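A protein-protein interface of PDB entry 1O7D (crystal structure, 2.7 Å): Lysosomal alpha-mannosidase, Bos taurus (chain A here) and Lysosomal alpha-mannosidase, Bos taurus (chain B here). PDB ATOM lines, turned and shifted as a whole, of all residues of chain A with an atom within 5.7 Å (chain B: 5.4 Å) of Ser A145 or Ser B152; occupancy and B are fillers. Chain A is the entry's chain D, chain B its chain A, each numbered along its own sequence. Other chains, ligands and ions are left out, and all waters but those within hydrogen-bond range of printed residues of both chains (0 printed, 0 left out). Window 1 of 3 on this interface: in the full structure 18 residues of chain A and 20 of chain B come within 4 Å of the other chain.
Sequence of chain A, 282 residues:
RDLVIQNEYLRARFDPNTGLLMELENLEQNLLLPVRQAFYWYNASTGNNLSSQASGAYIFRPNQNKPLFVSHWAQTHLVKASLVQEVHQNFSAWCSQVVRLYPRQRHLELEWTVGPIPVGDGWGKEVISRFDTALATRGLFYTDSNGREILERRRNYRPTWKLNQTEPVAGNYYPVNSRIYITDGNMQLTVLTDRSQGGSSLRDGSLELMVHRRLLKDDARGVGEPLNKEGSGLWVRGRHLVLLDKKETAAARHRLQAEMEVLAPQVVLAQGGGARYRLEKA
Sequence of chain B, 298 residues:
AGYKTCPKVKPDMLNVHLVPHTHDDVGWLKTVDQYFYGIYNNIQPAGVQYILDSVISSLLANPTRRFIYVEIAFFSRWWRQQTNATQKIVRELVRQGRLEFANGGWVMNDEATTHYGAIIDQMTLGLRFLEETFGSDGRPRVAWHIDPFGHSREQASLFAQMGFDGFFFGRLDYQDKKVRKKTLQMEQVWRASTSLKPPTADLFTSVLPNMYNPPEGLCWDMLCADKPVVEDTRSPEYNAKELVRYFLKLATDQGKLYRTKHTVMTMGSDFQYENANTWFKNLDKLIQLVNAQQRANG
Along chain A the printed residues that touch a printed residue of chain B span positions 145 to 151.
Among the printed residues, Asp or Glu carboxylates within 4 Å of a Lys or Arg side-chain nitrogen of the other chain: Glu A149 with Arg B153 (3.2 Å).
The side-chain amide oxygen (OD1) of Asn A146 lies close to the backbone carbonyl oxygen (O) of Glu B111, 3.2 Å away.
The side-chain hydroxyl of Ser B152 sits at hydrogen-bond distance from the side-chain amide nitrogen of Asn A146 (2.6 Å).
NH2 of Arg B153 is in salt-bridge range of OE1 of Glu A149 (3.2 Å).
The backbone NH (N) of Glu B154 sits at hydrogen-bond distance from the side-chain hydroxyl (OG) of Ser A145 (3.3 Å).
OE1 of Glu B154 lies within hydrogen-bond range of N of Glu A149 (3.3 Å).
The side-chain carboxylate of Glu B111 is in hydrogen-bond range of a ring nitrogen (ND1) of His B151.
The side-chain carboxylate of Glu B111 lies within hydrogen-bond range of the backbone NH of Ser B152, at 2.9 Å.
The backbone NH (N) of Gln B155 lies within hydrogen-bond range of the side-chain hydroxyl (OG) of Ser B152, 3.3 Å away.
N of Leu A151 lies within hydrogen-bond range of O of Thr A143, at 3.0 Å.
OD1 of Asn A146 lies close to ND2 of Asn A177.
Of the printed residues of chain B, Asn A146 touches Glu B111, Ser B152 and Glu B154.
Of the printed residues of chain B, Arg A148 touches Glu B154.
Of the printed residues of chain B, Glu A149 touches Arg B153 (3.2 Å) and Glu B154 (3.3 Å).
His B151 touches none of the printed residues of chain A.
Of the printed residues of chain A, Ser B152 touches Ser A145 and Asn A146.
Printed residues of chain A within 4 Å of Arg B153: Ser A145 (3.8 Å), Glu A149 (3.2 Å) and Leu A151 (3.0 Å).
Of the printed residues of chain A, Glu B154 touches Ser A145, Asn A146, Arg A148 and Glu A149.
The nearest printed residue of chain B that does not touch Asn A146 is Gln B155 (4.2 Å).
OG of Ser A145 touches CB of Ser B152, at 3.4 Å.
Arg B153 touches Ser A145 (N to OG, 3.8 Å).
CB of Glu B154 touches ND2 of Asn A146, at 3.7 Å.
Glu B154 touches Arg A148.
Leu A151 touches Arg B153.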
ATOM      1  N   THR A 143     -19.935 -19.265 -11.564  1.00  0.00           N
ATOM      2  CA  THR A 143     -20.134 -19.596 -10.163  1.00  0.00           C
ATOM      3  C   THR A 143     -21.614 -19.797  -9.890  1.00  0.00           C
ATOM      4  O   THR A 143     -22.471 -19.181 -10.533  1.00  0.00           O
ATOM      5  CB  THR A 143     -19.654 -18.453  -9.250  1.00  0.00           C
ATOM      6  OG1 THR A 143     -18.249 -18.244  -9.429  1.00  0.00           O
ATOM      7  CG2 THR A 143     -19.933 -18.788  -7.793  1.00  0.00           C
ATOM      8  N   ASP A 144     -21.916 -20.655  -8.927  1.00  0.00           N
ATOM      9  CA  ASP A 144     -23.302 -20.903  -8.578  1.00  0.00           C
ATOM     10  C   ASP A 144     -23.714 -19.983  -7.437  1.00  0.00           C
ATOM     11  O   ASP A 144     -22.943 -19.726  -6.525  1.00  0.00           O
ATOM     12  CB  ASP A 144     -23.506 -22.379  -8.182  1.00  0.00           C
ATOM     13  CG  ASP A 144     -22.801 -22.755  -6.877  1.00  0.00           C
ATOM     14  OD1 ASP A 144     -21.562 -22.966  -6.884  1.00  0.00           O
ATOM     15  OD2 ASP A 144     -23.498 -22.840  -5.837  1.00  0.00           O
ATOM     16  N   SER A 145     -24.932 -19.468  -7.501  1.00  0.00           N
ATOM     17  CA  SER A 145     -25.427 -18.600  -6.442  1.00  0.00           C
ATOM     18  C   SER A 145     -26.203 -19.467  -5.462  1.00  0.00           C
ATOM     19  O   SER A 145     -27.287 -19.944  -5.764  1.00  0.00           O
ATOM     20  CB  SER A 145     -26.339 -17.501  -7.020  1.00  0.00           C
ATOM     21  OG  SER A 145     -26.853 -16.612  -6.028  1.00  0.00           O
ATOM     22  N   ASN A 146     -25.639 -19.680  -4.285  1.00  0.00           N
ATOM     23  CA  ASN A 146     -26.303 -20.497  -3.279  1.00  0.00           C
ATOM     24  C   ASN A 146     -26.791 -21.834  -3.822  1.00  0.00           C
ATOM     25  O   ASN A 146     -27.803 -22.366  -3.372  1.00  0.00           O
ATOM     26  CB  ASN A 146     -27.466 -19.730  -2.662  1.00  0.00           C
ATOM     27  CG  ASN A 146     -27.015 -18.494  -1.938  1.00  0.00           C
ATOM     28  OD1 ASN A 146     -26.104 -18.545  -1.112  1.00  0.00           O
ATOM     29  ND2 ASN A 146     -27.645 -17.372  -2.240  1.00  0.00           N
ATOM     30  N   GLY A 147     -26.067 -22.361  -4.809  1.00  0.00           N
ATOM     31  CA  GLY A 147     -26.386 -23.663  -5.393  1.00  0.00           C
ATOM     32  C   GLY A 147     -27.544 -23.752  -6.375  1.00  0.00           C
ATOM     33  O   GLY A 147     -28.081 -24.830  -6.569  1.00  0.00           O
ATOM     34  N   ARG A 148     -27.932 -22.645  -7.009  1.00  0.00           N
ATOM     35  CA  ARG A 148     -29.052 -22.681  -7.954  1.00  0.00           C
ATOM     36  C   ARG A 148     -28.681 -22.235  -9.350  1.00  0.00           C
ATOM     37  O   ARG A 148     -28.043 -22.987 -10.091  1.00  0.00           O
ATOM     38  CB  ARG A 148     -30.224 -21.837  -7.450  1.00  0.00           C
ATOM     39  CG  ARG A 148     -30.794 -22.345  -6.145  1.00  0.00           C
ATOM     40  CD  ARG A 148     -32.302 -22.261  -6.131  1.00  0.00           C
ATOM     41  NE  ARG A 148     -32.890 -23.147  -7.124  1.00  0.00           N
ATOM     42  CZ  ARG A 148     -34.187 -23.196  -7.417  1.00  0.00           C
ATOM     43  NH1 ARG A 148     -35.056 -22.409  -6.798  1.00  0.00           N
ATOM     44  NH2 ARG A 148     -34.619 -24.042  -8.336  1.00  0.00           N
ATOM     45  N   GLU A 149     -29.084 -21.021  -9.714  1.00  0.00           N
ATOM     46  CA  GLU A 149     -28.755 -20.511 -11.033  1.00  0.00           C
ATOM     47  C   GLU A 149     -27.274 -20.107 -11.049  1.00  0.00           C
ATOM     48  O   GLU A 149     -26.694 -19.831 -10.000  1.00  0.00           O
ATOM     49  CB  GLU A 149     -29.678 -19.342 -11.390  1.00  0.00           C
ATOM     50  CG  GLU A 149     -31.155 -19.768 -11.440  1.00  0.00           C
ATOM     51  CD  GLU A 149     -32.086 -18.673 -11.917  1.00  0.00           C
ATOM     52  OE1 GLU A 149     -31.804 -18.102 -12.987  1.00  0.00           O
ATOM     53  OE2 GLU A 149     -33.094 -18.398 -11.220  1.00  0.00           O
ATOM     54  N   ILE A 150     -26.658 -20.105 -12.230  1.00  0.00           N
ATOM     55  CA  ILE A 150     -25.247 -19.763 -12.346  1.00  0.00           C
ATOM     56  C   ILE A 150     -25.028 -18.380 -12.977  1.00  0.00           C
ATOM     57  O   ILE A 150     -25.591 -18.068 -14.016  1.00  0.00           O
ATOM     58  CB  ILE A 150     -24.510 -20.847 -13.157  1.00  0.00           C
ATOM     59  CG1 ILE A 150     -24.848 -22.216 -12.580  1.00  0.00           C
ATOM     60  CG2 ILE A 150     -23.011 -20.637 -13.092  1.00  0.00           C
ATOM     61  CD1 ILE A 150     -24.033 -23.353 -13.169  1.00  0.00           C
ATOM     62  N   LEU A 151     -24.207 -17.561 -12.327  1.00  0.00           N
ATOM     63  CA  LEU A 151     -23.916 -16.208 -12.798  1.00  0.00           C
ATOM     64  C   LEU A 151     -22.537 -16.118 -13.456  1.00  0.00           C
ATOM     65  O   LEU A 151     -21.557 -16.662 -12.942  1.00  0.00           O
ATOM     66  CB  LEU A 151     -23.995 -15.222 -11.627  1.00  0.00           C
ATOM     67  CG  LEU A 151     -25.252 -15.375 -10.770  1.00  0.00           C
ATOM     68  CD1 LEU A 151     -25.291 -14.349  -9.651  1.00  0.00           C
ATOM     69  CD2 LEU A 151     -26.451 -15.227 -11.667  1.00  0.00           C
ATOM     70  N   ASN A 177     -20.616 -21.792  -3.659  1.00  0.00           N
ATOM     71  CA  ASN A 177     -21.226 -22.686  -2.690  1.00  0.00           C
ATOM     72  C   ASN A 177     -21.309 -24.142  -3.100  1.00  0.00           C
ATOM     73  O   ASN A 177     -21.437 -25.019  -2.234  1.00  0.00           O
ATOM     74  CB  ASN A 177     -22.643 -22.216  -2.336  1.00  0.00           C
ATOM     75  CG  ASN A 177     -22.665 -20.819  -1.763  1.00  0.00           C
ATOM     76  OD1 ASN A 177     -21.697 -20.360  -1.164  1.00  0.00           O
ATOM     77  ND2 ASN A 177     -23.778 -20.138  -1.931  1.00  0.00           N
ATOM     78  N   GLU B 111     -25.711 -14.262   2.901  1.00  0.00           N
ATOM     79  CA  GLU B 111     -26.020 -14.590   1.517  1.00  0.00           C
ATOM     80  C   GLU B 111     -24.894 -15.190   0.676  1.00  0.00           C
ATOM     81  O   GLU B 111     -25.120 -15.581  -0.470  1.00  0.00           O
ATOM     82  CB  GLU B 111     -26.572 -13.345   0.805  1.00  0.00           C
ATOM     83  CG  GLU B 111     -27.892 -12.815   1.386  1.00  0.00           C
ATOM     84  CD  GLU B 111     -28.397 -11.533   0.706  1.00  0.00           C
ATOM     85  OE1 GLU B 111     -28.454 -11.510  -0.544  1.00  0.00           O
ATOM     86  OE2 GLU B 111     -28.743 -10.564   1.422  1.00  0.00           O
ATOM     87  N   GLY B 150     -22.937  -8.070   1.056  1.00  0.00           N
ATOM     88  CA  GLY B 150     -23.115  -8.287  -0.368  1.00  0.00           C
ATOM     89  C   GLY B 150     -24.385  -9.091  -0.512  1.00  0.00           C
ATOM     90  O   GLY B 150     -24.851  -9.670   0.462  1.00  0.00           O
ATOM     91  N   HIS B 151     -24.948  -9.158  -1.708  1.00  0.00           N
ATOM     92  CA  HIS B 151     -26.204  -9.871  -1.866  1.00  0.00           C
ATOM     93  C   HIS B 151     -26.224 -10.773  -3.078  1.00  0.00           C
ATOM     94  O   HIS B 151     -25.743 -10.390  -4.148  1.00  0.00           O
ATOM     95  CB  HIS B 151     -27.335  -8.847  -1.925  1.00  0.00           C
ATOM     96  CG  HIS B 151     -27.293  -7.867  -0.797  1.00  0.00           C
ATOM     97  ND1 HIS B 151     -27.796  -8.152   0.454  1.00  0.00           N
ATOM     98  CD2 HIS B 151     -26.688  -6.660  -0.692  1.00  0.00           C
ATOM     99  CE1 HIS B 151     -27.498  -7.166   1.283  1.00  0.00           C
ATOM    100  NE2 HIS B 151     -26.824  -6.249   0.612  1.00  0.00           N
ATOM    101  N   SER B 152     -26.783 -11.972  -2.900  1.00  0.00           N
ATOM    102  CA  SER B 152     -26.861 -12.949  -3.981  1.00  0.00           C
ATOM    103  C   SER B 152     -28.168 -12.839  -4.744  1.00  0.00           C
ATOM    104  O   SER B 152     -29.216 -12.545  -4.164  1.00  0.00           O
ATOM    105  CB  SER B 152     -26.704 -14.379  -3.440  1.00  0.00           C
ATOM    106  OG  SER B 152     -27.785 -14.771  -2.607  1.00  0.00           O
ATOM    107  N   ARG B 153     -28.105 -13.073  -6.048  1.00  0.00           N
ATOM    108  CA  ARG B 153     -29.306 -13.001  -6.853  1.00  0.00           C
ATOM    109  C   ARG B 153     -30.316 -14.066  -6.415  1.00  0.00           C
ATOM    110  O   ARG B 153     -31.527 -13.853  -6.504  1.00  0.00           O
ATOM    111  CB  ARG B 153     -28.985 -13.171  -8.335  1.00  0.00           C
ATOM    112  CG  ARG B 153     -30.126 -12.696  -9.197  1.00  0.00           C
ATOM    113  CD  ARG B 153     -29.854 -12.879 -10.660  1.00  0.00           C
ATOM    114  NE  ARG B 153     -29.792 -14.287 -11.035  1.00  0.00           N
ATOM    115  CZ  ARG B 153     -29.391 -14.723 -12.226  1.00  0.00           C
ATOM    116  NH1 ARG B 153     -29.011 -13.856 -13.158  1.00  0.00           N
ATOM    117  NH2 ARG B 153     -29.367 -16.027 -12.491  1.00  0.00           N
ATOM    118  N   GLU B 154     -29.831 -15.206  -5.924  1.00  0.00           N
ATOM    119  CA  GLU B 154     -30.744 -16.261  -5.506  1.00  0.00           C
ATOM    120  C   GLU B 154     -31.606 -15.801  -4.323  1.00  0.00           C
ATOM    121  O   GLU B 154     -32.816 -16.049  -4.291  1.00  0.00           O
ATOM    122  CB  GLU B 154     -29.970 -17.526  -5.153  1.00  0.00           C
ATOM    123  CG  GLU B 154     -30.827 -18.776  -5.206  1.00  0.00           C
ATOM    124  CD  GLU B 154     -31.446 -19.008  -6.597  1.00  0.00           C
ATOM    125  OE1 GLU B 154     -30.689 -19.084  -7.586  1.00  0.00           O
ATOM    126  OE2 GLU B 154     -32.687 -19.122  -6.718  1.00  0.00           O
ATOM    127  N   GLN B 155     -30.988 -15.125  -3.356  1.00  0.00           N
ATOM    128  CA  GLN B 155     -31.725 -14.606  -2.211  1.00  0.00           C
ATOM    129  C   GLN B 155     -32.954 -13.825  -2.702  1.00  0.00           C
ATOM    130  O   GLN B 155     -34.070 -14.043  -2.240  1.00  0.00           O
ATOM    131  CB  GLN B 155     -30.830 -13.674  -1.394  1.00  0.00           C
ATOM    132  CG  GLN B 155     -31.436 -13.195  -0.081  1.00  0.00           C
ATOM    133  CD  GLN B 155     -31.759 -14.349   0.854  1.00  0.00           C
ATOM    134  OE1 GLN B 155     -32.174 -14.157   2.005  1.00  0.00           O
ATOM    135  NE2 GLN B 155     -31.574 -15.566   0.357  1.00  0.00           N
ATOM    136  N   ALA B 156     -32.743 -12.916  -3.647  1.00  0.00           N
ATOM    137  CA  ALA B 156     -33.835 -12.117  -4.173  1.00  0.00           C
ATOM    138  C   ALA B 156     -34.906 -13.019  -4.771  1.00  0.00           C
ATOM    139  O   ALA B 156     -36.098 -12.799  -4.577  1.00  0.00           O
ATOM    140  CB  ALA B 156     -33.310 -11.149  -5.212  1.00  0.00           C
ATOM    141  N   TRP B 190     -35.329  -5.756  -9.049  1.00  0.00           N
ATOM    142  CA  TRP B 190     -34.327  -6.782  -9.258  1.00  0.00           C
ATOM    143  C   TRP B 190     -34.887  -8.087  -9.850  1.00  0.00           C
ATOM    144  O   TRP B 190     -35.667  -8.798  -9.198  1.00  0.00           O
ATOM    145  CB  TRP B 190     -33.613  -7.064  -7.926  1.00  0.00           C
ATOM    146  CG  TRP B 190     -32.345  -7.881  -8.038  1.00  0.00           C
ATOM    147  CD1 TRP B 190     -31.814  -8.423  -9.173  1.00  0.00           C
ATOM    148  CD2 TRP B 190     -31.477  -8.272  -6.964  1.00  0.00           C
ATOM    149  NE1 TRP B 190     -30.672  -9.133  -8.876  1.00  0.00           N
ATOM    150  CE2 TRP B 190     -30.442  -9.057  -7.528  1.00  0.00           C
ATOM    151  CE3 TRP B 190     -31.475  -8.039  -5.582  1.00  0.00           C
ATOM    152  CZ2 TRP B 190     -29.415  -9.608  -6.758  1.00  0.00           C
ATOM    153  CZ3 TRP B 190     -30.461  -8.587  -4.821  1.00  0.00           C
ATOM    154  CH2 TRP B 190     -29.440  -9.366  -5.412  1.00  0.00           C
